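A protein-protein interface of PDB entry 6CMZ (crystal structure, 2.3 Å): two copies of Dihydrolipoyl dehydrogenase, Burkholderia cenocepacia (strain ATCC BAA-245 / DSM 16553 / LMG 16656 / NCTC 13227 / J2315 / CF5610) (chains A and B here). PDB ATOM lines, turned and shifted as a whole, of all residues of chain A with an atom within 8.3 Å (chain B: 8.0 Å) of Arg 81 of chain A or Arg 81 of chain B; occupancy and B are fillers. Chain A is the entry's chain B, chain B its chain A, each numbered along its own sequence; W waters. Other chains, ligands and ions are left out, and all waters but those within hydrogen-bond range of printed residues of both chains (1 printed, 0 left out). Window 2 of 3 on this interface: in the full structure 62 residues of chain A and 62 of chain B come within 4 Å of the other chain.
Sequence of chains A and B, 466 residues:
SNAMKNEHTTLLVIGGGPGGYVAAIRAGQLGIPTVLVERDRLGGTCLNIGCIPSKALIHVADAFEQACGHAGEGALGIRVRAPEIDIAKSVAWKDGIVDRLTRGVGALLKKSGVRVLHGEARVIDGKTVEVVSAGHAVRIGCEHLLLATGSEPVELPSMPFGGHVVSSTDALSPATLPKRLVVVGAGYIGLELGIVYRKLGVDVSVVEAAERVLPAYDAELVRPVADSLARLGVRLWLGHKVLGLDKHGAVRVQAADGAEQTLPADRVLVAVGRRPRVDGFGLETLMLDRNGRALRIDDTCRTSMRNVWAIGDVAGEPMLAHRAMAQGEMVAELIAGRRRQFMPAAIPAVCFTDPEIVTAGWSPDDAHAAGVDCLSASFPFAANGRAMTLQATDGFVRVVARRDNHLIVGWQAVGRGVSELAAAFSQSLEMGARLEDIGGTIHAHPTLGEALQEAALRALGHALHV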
ATOM      1  N   GLN A  66      26.455   0.759 -12.317  1.00  0.00           N
ATOM      2  CA  GLN A  66      25.663  -0.266 -13.014  1.00  0.00           C
ATOM      3  C   GLN A  66      24.256  -0.382 -12.441  1.00  0.00           C
ATOM      4  O   GLN A  66      23.288  -0.500 -13.188  1.00  0.00           O
ATOM      5  CB  GLN A  66      26.396  -1.598 -12.955  1.00  0.00           C
ATOM      6  CG  GLN A  66      27.720  -1.544 -13.712  1.00  0.00           C
ATOM      7  CD  GLN A  66      28.680  -2.641 -13.314  1.00  0.00           C
ATOM      8  OE1 GLN A  66      28.301  -3.606 -12.657  1.00  0.00           O
ATOM      9  NE2 GLN A  66      29.948  -2.477 -13.689  1.00  0.00           N
ATOM     10  N   ALA A  67      24.141  -0.315 -11.121  1.00  0.00           N
ATOM     11  CA  ALA A  67      22.834  -0.369 -10.463  1.00  0.00           C
ATOM     12  C   ALA A  67      21.961   0.821 -10.898  1.00  0.00           C
ATOM     13  O   ALA A  67      20.736   0.686 -11.023  1.00  0.00           O
ATOM     14  CB  ALA A  67      22.999  -0.389  -8.954  1.00  0.00           C
ATOM     15  N   CYS A  68      22.598   1.972 -11.129  1.00  0.00           N
ATOM     16  CA  CYS A  68      21.900   3.193 -11.580  1.00  0.00           C
ATOM     17  C   CYS A  68      21.570   3.153 -13.066  1.00  0.00           C
ATOM     18  O   CYS A  68      20.895   4.049 -13.564  1.00  0.00           O
ATOM     19  CB  CYS A  68      22.751   4.457 -11.344  1.00  0.00           C
ATOM     20  SG  CYS A  68      23.039   4.957  -9.632  1.00  0.00           S
ATOM     21  N   GLY A  69      22.073   2.143 -13.772  1.00  0.00           N
ATOM     22  CA  GLY A  69      21.848   2.024 -15.203  1.00  0.00           C
ATOM     23  C   GLY A  69      22.709   2.973 -16.021  1.00  0.00           C
ATOM     24  O   GLY A  69      22.390   3.255 -17.187  1.00  0.00           O
ATOM     25  N   ILE A  78      17.443  -3.961 -20.017  1.00  0.00           N
ATOM     26  CA  ILE A  78      17.267  -3.891 -18.564  1.00  0.00           C
ATOM     27  C   ILE A  78      16.869  -2.477 -18.158  1.00  0.00           C
ATOM     28  O   ILE A  78      17.651  -1.537 -18.265  1.00  0.00           O
ATOM     29  CB  ILE A  78      18.537  -4.336 -17.805  1.00  0.00           C
ATOM     30  CG1 ILE A  78      18.952  -5.741 -18.254  1.00  0.00           C
ATOM     31  CG2 ILE A  78      18.306  -4.304 -16.296  1.00  0.00           C
ATOM     32  CD1 ILE A  78      20.217  -6.258 -17.595  1.00  0.00           C
ATOM     33  N   ARG A  79      15.638  -2.350 -17.689  1.00  0.00           N
ATOM     34  CA  ARG A  79      15.092  -1.080 -17.260  1.00  0.00           C
ATOM     35  C   ARG A  79      15.243  -1.119 -15.742  1.00  0.00           C
ATOM     36  O   ARG A  79      14.708  -2.003 -15.076  1.00  0.00           O
ATOM     37  CB  ARG A  79      13.656  -0.995 -17.754  1.00  0.00           C
ATOM     38  CG  ARG A  79      13.026   0.384 -17.804  1.00  0.00           C
ATOM     39  CD  ARG A  79      11.818   0.321 -18.744  1.00  0.00           C
ATOM     40  NE  ARG A  79      10.980   1.526 -18.732  1.00  0.00           N
ATOM     41  CZ  ARG A  79       9.895   1.706 -17.972  1.00  0.00           C
ATOM     42  NH1 ARG A  79       9.218   2.849 -18.064  1.00  0.00           N
ATOM     43  NH2 ARG A  79       9.467   0.764 -17.125  1.00  0.00           N
ATOM     44  N   VAL A  80      16.017  -0.179 -15.213  1.00  0.00           N
ATOM     45  CA  VAL A  80      16.320  -0.133 -13.780  1.00  0.00           C
ATOM     46  C   VAL A  80      15.587   0.969 -13.038  1.00  0.00           C
ATOM     47  O   VAL A  80      15.047   1.893 -13.649  1.00  0.00           O
ATOM     48  CB  VAL A  80      17.834   0.121 -13.550  1.00  0.00           C
ATOM     49  CG1 VAL A  80      18.672  -0.912 -14.282  1.00  0.00           C
ATOM     50  CG2 VAL A  80      18.257   1.522 -14.001  1.00  0.00           C
ATOM     51  N   ARG A  81      15.586   0.861 -11.712  1.00  0.00           N
ATOM     52  CA  ARG A  81      15.014   1.891 -10.853  1.00  0.00           C
ATOM     53  C   ARG A  81      16.141   2.296  -9.905  1.00  0.00           C
ATOM     54  O   ARG A  81      16.918   1.447  -9.455  1.00  0.00           O
ATOM     55  CB  ARG A  81      13.770   1.422 -10.100  1.00  0.00           C
ATOM     56  CG  ARG A  81      13.056   2.577  -9.399  1.00  0.00           C
ATOM     57  CD  ARG A  81      11.824   2.135  -8.624  1.00  0.00           C
ATOM     58  NE  ARG A  81      10.744   1.636  -9.474  1.00  0.00           N
ATOM     59  CZ  ARG A  81       9.545   1.256  -9.026  1.00  0.00           C
ATOM     60  NH1 ARG A  81       9.249   1.319  -7.728  1.00  0.00           N
ATOM     61  NH2 ARG A  81       8.626   0.818  -9.884  1.00  0.00           N
ATOM     62  N   ALA A  82      16.224   3.596  -9.627  1.00  0.00           N
ATOM     63  CA  ALA A  82      17.286   4.190  -8.793  1.00  0.00           C
ATOM     64  C   ALA A  82      17.609   3.440  -7.492  1.00  0.00           C
ATOM     65  O   ALA A  82      16.709   3.116  -6.723  1.00  0.00           O
ATOM     66  CB  ALA A  82      16.940   5.639  -8.470  1.00  0.00           C
ATOM     67  N   PRO A  83      18.898   3.137  -7.261  1.00  0.00           N
ATOM     68  CA  PRO A  83      19.311   2.494  -6.028  1.00  0.00           C
ATOM     69  C   PRO A  83      19.797   3.542  -5.022  1.00  0.00           C
ATOM     70  O   PRO A  83      19.776   4.742  -5.309  1.00  0.00           O
ATOM     71  CB  PRO A  83      20.462   1.615  -6.483  1.00  0.00           C
ATOM     72  CG  PRO A  83      21.099   2.407  -7.558  1.00  0.00           C
ATOM     73  CD  PRO A  83      19.994   3.146  -8.247  1.00  0.00           C
ATOM     74  N   GLU A  84      20.229   3.083  -3.853  1.00  0.00           N
ATOM     75  CA  GLU A  84      20.733   3.968  -2.806  1.00  0.00           C
ATOM     76  C   GLU A  84      22.029   3.427  -2.265  1.00  0.00           C
ATOM     77  O   GLU A  84      22.199   2.211  -2.186  1.00  0.00           O
ATOM     78  CB  GLU A  84      19.739   4.061  -1.654  1.00  0.00           C
ATOM     79  CG  GLU A  84      18.438   4.753  -1.988  1.00  0.00           C
ATOM     80  CD  GLU A  84      17.468   4.742  -0.820  1.00  0.00           C
ATOM     81  OE1 GLU A  84      17.674   3.952   0.133  1.00  0.00           O
ATOM     82  OE2 GLU A  84      16.485   5.511  -0.859  1.00  0.00           O
ATOM     83  N   GLN B  66      23.218  -8.563 -11.189  1.00  0.00           N
ATOM     84  CA  GLN B  66      23.765  -7.439 -10.454  1.00  0.00           C
ATOM     85  C   GLN B  66      22.716  -6.366 -10.176  1.00  0.00           C
ATOM     86  O   GLN B  66      22.700  -5.804  -9.098  1.00  0.00           O
ATOM     87  CB  GLN B  66      24.987  -6.866 -11.189  1.00  0.00           C
ATOM     88  CG  GLN B  66      26.162  -7.842 -11.157  1.00  0.00           C
ATOM     89  CD  GLN B  66      27.280  -7.504 -12.126  1.00  0.00           C
ATOM     90  OE1 GLN B  66      27.393  -6.377 -12.601  1.00  0.00           O
ATOM     91  NE2 GLN B  66      28.101  -8.497 -12.436  1.00  0.00           N
ATOM     92  N   ALA B  67      21.835  -6.107 -11.134  1.00  0.00           N
ATOM     93  CA  ALA B  67      20.790  -5.117 -10.952  1.00  0.00           C
ATOM     94  C   ALA B  67      19.817  -5.552  -9.843  1.00  0.00           C
ATOM     95  O   ALA B  67      19.315  -4.705  -9.091  1.00  0.00           O
ATOM     96  CB  ALA B  67      20.064  -4.881 -12.260  1.00  0.00           C
ATOM     97  N   CYS B  68      19.588  -6.868  -9.738  1.00  0.00           N
ATOM     98  CA  CYS B  68      18.703  -7.459  -8.710  1.00  0.00           C
ATOM     99  C   CYS B  68      19.334  -7.596  -7.305  1.00  0.00           C
ATOM    100  O   CYS B  68      18.624  -7.904  -6.331  1.00  0.00           O
ATOM    101  CB  CYS B  68      18.224  -8.858  -9.133  1.00  0.00           C
ATOM    102  SG  CYS B  68      17.171  -8.954 -10.597  1.00  0.00           S
ATOM    103  N   GLY B  69      20.646  -7.386  -7.198  1.00  0.00           N
ATOM    104  CA  GLY B  69      21.336  -7.515  -5.922  1.00  0.00           C
ATOM    105  C   GLY B  69      21.660  -8.961  -5.570  1.00  0.00           C
ATOM    106  O   GLY B  69      21.786  -9.301  -4.400  1.00  0.00           O
ATOM    107  N   ILE B  78      25.133  -0.993  -1.051  1.00  0.00           N
ATOM    108  CA  ILE B  78      24.209  -0.642  -2.124  1.00  0.00           C
ATOM    109  C   ILE B  78      22.875  -1.358  -1.944  1.00  0.00           C
ATOM    110  O   ILE B  78      22.813  -2.587  -1.958  1.00  0.00           O
ATOM    111  CB  ILE B  78      24.791  -0.992  -3.500  1.00  0.00           C
ATOM    112  CG1 ILE B  78      26.128  -0.268  -3.701  1.00  0.00           C
ATOM    113  CG2 ILE B  78      23.797  -0.634  -4.598  1.00  0.00           C
ATOM    114  CD1 ILE B  78      26.851  -0.640  -4.979  1.00  0.00           C
ATOM    115  N   ARG B  79      21.813  -0.572  -1.786  1.00  0.00           N
ATOM    116  CA  ARG B  79      20.458  -1.087  -1.591  1.00  0.00           C
ATOM    117  C   ARG B  79      19.734  -0.862  -2.915  1.00  0.00           C
ATOM    118  O   ARG B  79      19.654   0.269  -3.402  1.00  0.00           O
ATOM    119  CB  ARG B  79      19.817  -0.349  -0.414  1.00  0.00           C
ATOM    120  CG  ARG B  79      18.505  -0.900   0.109  1.00  0.00           C
ATOM    121  CD  ARG B  79      18.280  -0.374   1.525  1.00  0.00           C
ATOM    122  NE  ARG B  79      17.034  -0.849   2.138  1.00  0.00           N
ATOM    123  CZ  ARG B  79      15.926  -0.124   2.343  1.00  0.00           C
ATOM    124  NH1 ARG B  79      14.870  -0.696   2.920  1.00  0.00           N
ATOM    125  NH2 ARG B  79      15.858   1.167   2.010  1.00  0.00           N
ATOM    126  N   VAL B  80      19.238  -1.946  -3.509  1.00  0.00           N
ATOM    127  CA  VAL B  80      18.583  -1.862  -4.816  1.00  0.00           C
ATOM    128  C   VAL B  80      17.087  -2.080  -4.801  1.00  0.00           C
ATOM    129  O   VAL B  80      16.521  -2.568  -3.831  1.00  0.00           O
ATOM    130  CB  VAL B  80      19.147  -2.912  -5.809  1.00  0.00           C
ATOM    131  CG1 VAL B  80      20.627  -2.692  -6.016  1.00  0.00           C
ATOM    132  CG2 VAL B  80      18.870  -4.342  -5.337  1.00  0.00           C
ATOM    133  N   ARG B  81      16.484  -1.681  -5.916  1.00  0.00           N
ATOM    134  CA  ARG B  81      15.086  -1.890  -6.211  1.00  0.00           C
ATOM    135  C   ARG B  81      15.137  -2.818  -7.422  1.00  0.00           C
ATOM    136  O   ARG B  81      15.967  -2.626  -8.330  1.00  0.00           O
ATOM    137  CB  ARG B  81      14.375  -0.587  -6.522  1.00  0.00           C
ATOM    138  CG  ARG B  81      14.246   0.306  -5.309  1.00  0.00           C
ATOM    139  CD  ARG B  81      13.616   1.636  -5.658  1.00  0.00           C
ATOM    140  NE  ARG B  81      13.537   2.508  -4.490  1.00  0.00           N
ATOM    141  CZ  ARG B  81      13.245   3.804  -4.526  1.00  0.00           C
ATOM    142  NH1 ARG B  81      13.023   4.425  -5.689  1.00  0.00           N
ATOM    143  NH2 ARG B  81      13.202   4.495  -3.389  1.00  0.00           N
ATOM    144  N   ALA B  82      14.272  -3.831  -7.411  1.00  0.00           N
ATOM    145  CA  ALA B  82      14.231  -4.842  -8.465  1.00  0.00           C
ATOM    146  C   ALA B  82      14.018  -4.248  -9.857  1.00  0.00           C
ATOM    147  O   ALA B  82      13.220  -3.316 -10.025  1.00  0.00           O
ATOM    148  CB  ALA B  82      13.149  -5.869  -8.169  1.00  0.00           C
ATOM    149  N   PRO B  83      14.756  -4.766 -10.850  1.00  0.00           N
ATOM    150  CA  PRO B  83      14.620  -4.329 -12.227  1.00  0.00           C
ATOM    151  C   PRO B  83      13.664  -5.237 -12.993  1.00  0.00           C
ATOM    152  O   PRO B  83      13.193  -6.239 -12.453  1.00  0.00           O
ATOM    153  CB  PRO B  83      16.027  -4.522 -12.772  1.00  0.00           C
ATOM    154  CG  PRO B  83      16.518  -5.734 -12.054  1.00  0.00           C
ATOM    155  CD  PRO B  83      15.907  -5.675 -10.683  1.00  0.00           C
ATOM    156  N   GLU B  84      13.370  -4.863 -14.233  1.00  0.00           N
ATOM    157  CA  GLU B  84      12.547  -5.675 -15.126  1.00  0.00           C
ATOM    158  C   GLU B  84      13.394  -5.843 -16.375  1.00  0.00           C
ATOM    159  O   GLU B  84      14.277  -5.015 -16.642  1.00  0.00           O
ATOM    160  CB  GLU B  84      11.203  -5.009 -15.446  1.00  0.00           C
ATOM    161  CG  GLU B  84      11.288  -3.744 -16.297  1.00  0.00           C
ATOM    162  CD  GLU B  84       9.933  -3.112 -16.553  1.00  0.00           C
ATOM    163  OE1 GLU B  84       9.834  -2.296 -17.499  1.00  0.00           O
ATOM    164  OE2 GLU B  84       8.965  -3.434 -15.823  1.00  0.00           O
HETATM  165  O   HOH W   1      17.162  -1.818 -10.666  1.00  0.00           O
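CA of Ile 78 of chain A touches O of Glu 84 of chain B, at 3.7 Å. O of Arg 79 of chain A touches CB of Pro 83 of chain B (3.7 Å). CD of Arg 81 of chain A touches CD of Arg 81 of chain B, at 3.5 Å. Ala 82 of chain A touches Arg 81 of chain B. O of Arg 79 of chain B touches CB of Pro 83 of chain A (3.5 Å). Glu 84 of chain A touches Ile 78 of chain B.
Of the printed residues of chain B, Arg 79 of chain A touches Pro 83 (3.7 Å) and Glu 84 (3.1 Å). Arg 81 of chain A touches one residue of chain B. Ala 82 of chain A touches just one residue of chain B: Arg 81. Of the printed residues of chain A, Gln 66 of chain B touches Gln 66. Gly 69 of chain B touches none of the printed residues of chain A. Printed residues of chain A within 4 Å of Arg 79 of chain B: Pro 83 (3.5 Å) and Glu 84 (2.8 Å). Of chain A, only Arg 81 and Ala 82 come within 4 Å of Arg 81 of chain B. No residue of chain A comes within 4 Å of Ala 82 of chain B. Of the printed residues of chain A, Pro 83 of chain B touches Arg 79. Of the printed residues of chain A, Glu 84 of chain B touches Ile 78 (3.7 Å) and Arg 79 (3.1 Å). The nearest residue of chain B that does not touch Arg 81 of chain A is Ala 82 of chain B (4.8 Å).
Printed residues of chain A that touch a printed residue of chain B: Gln 66, Ile 78, Arg 79, Arg 81, Ala 82, Pro 83 and Glu 84. Hydrophobic or aromatic side chains of chain A within 4 Å of the printed part of chain B: Pro 83. Of the 11 printed residues of chain B, 6 touch a printed residue of chain A. Along chain B the printed residues that touch a printed residue of chain A span positions 66 to 84. Among the printed residues, 9 pairs touch across the chains. Among the printed residues, Asp or Glu carboxylates within 4 Å of a Lys or Arg side-chain nitrogen of the other chain: Arg 79 of chain A with Glu 84 of chain B and Glu 84 of chain A with Arg 79 of chain B.
Water W1 lies within hydrogen-bond range of the backbone carbonyl oxygen (O) of Arg 81 of chain B and the backbone NH (N) of Arg 81 of chain A.
Gln 66 of chain B touches its own counterpart, Gln 66 of chain A. Arg 79 of chain A touches Pro 83 of chain B, and with the chains exchanged Pro 83 of chain A touches Arg 79 of chain B. Arg 81 of chain B touches its own counterpart, Arg 81 of chain A. Ala 82 of chain A touches Arg 81 of chain B, but with the chains exchanged Arg 81 of chain A does not touch Ala 82 of chain B (4.8 Å). Positions printed for both chains: 66, 67, 68, 69, 78, 79, 80, 81, 82, 83 and 84. Of the 9 pairs that touch across the chains among the printed residues, 8 have their exchanged pair printed and touching as well.
OE1 of Gln 66 of chain B lies close to OE1 of Gln 66 of chain A (2.9 Å). NH2 of Arg 79 of chain B lies within salt-bridge range of OE1 of Glu 84 of chain A. NH2 of Arg 79 of chain A is in salt-bridge range of OE1 of Glu 84 of chain B (3.1 Å).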
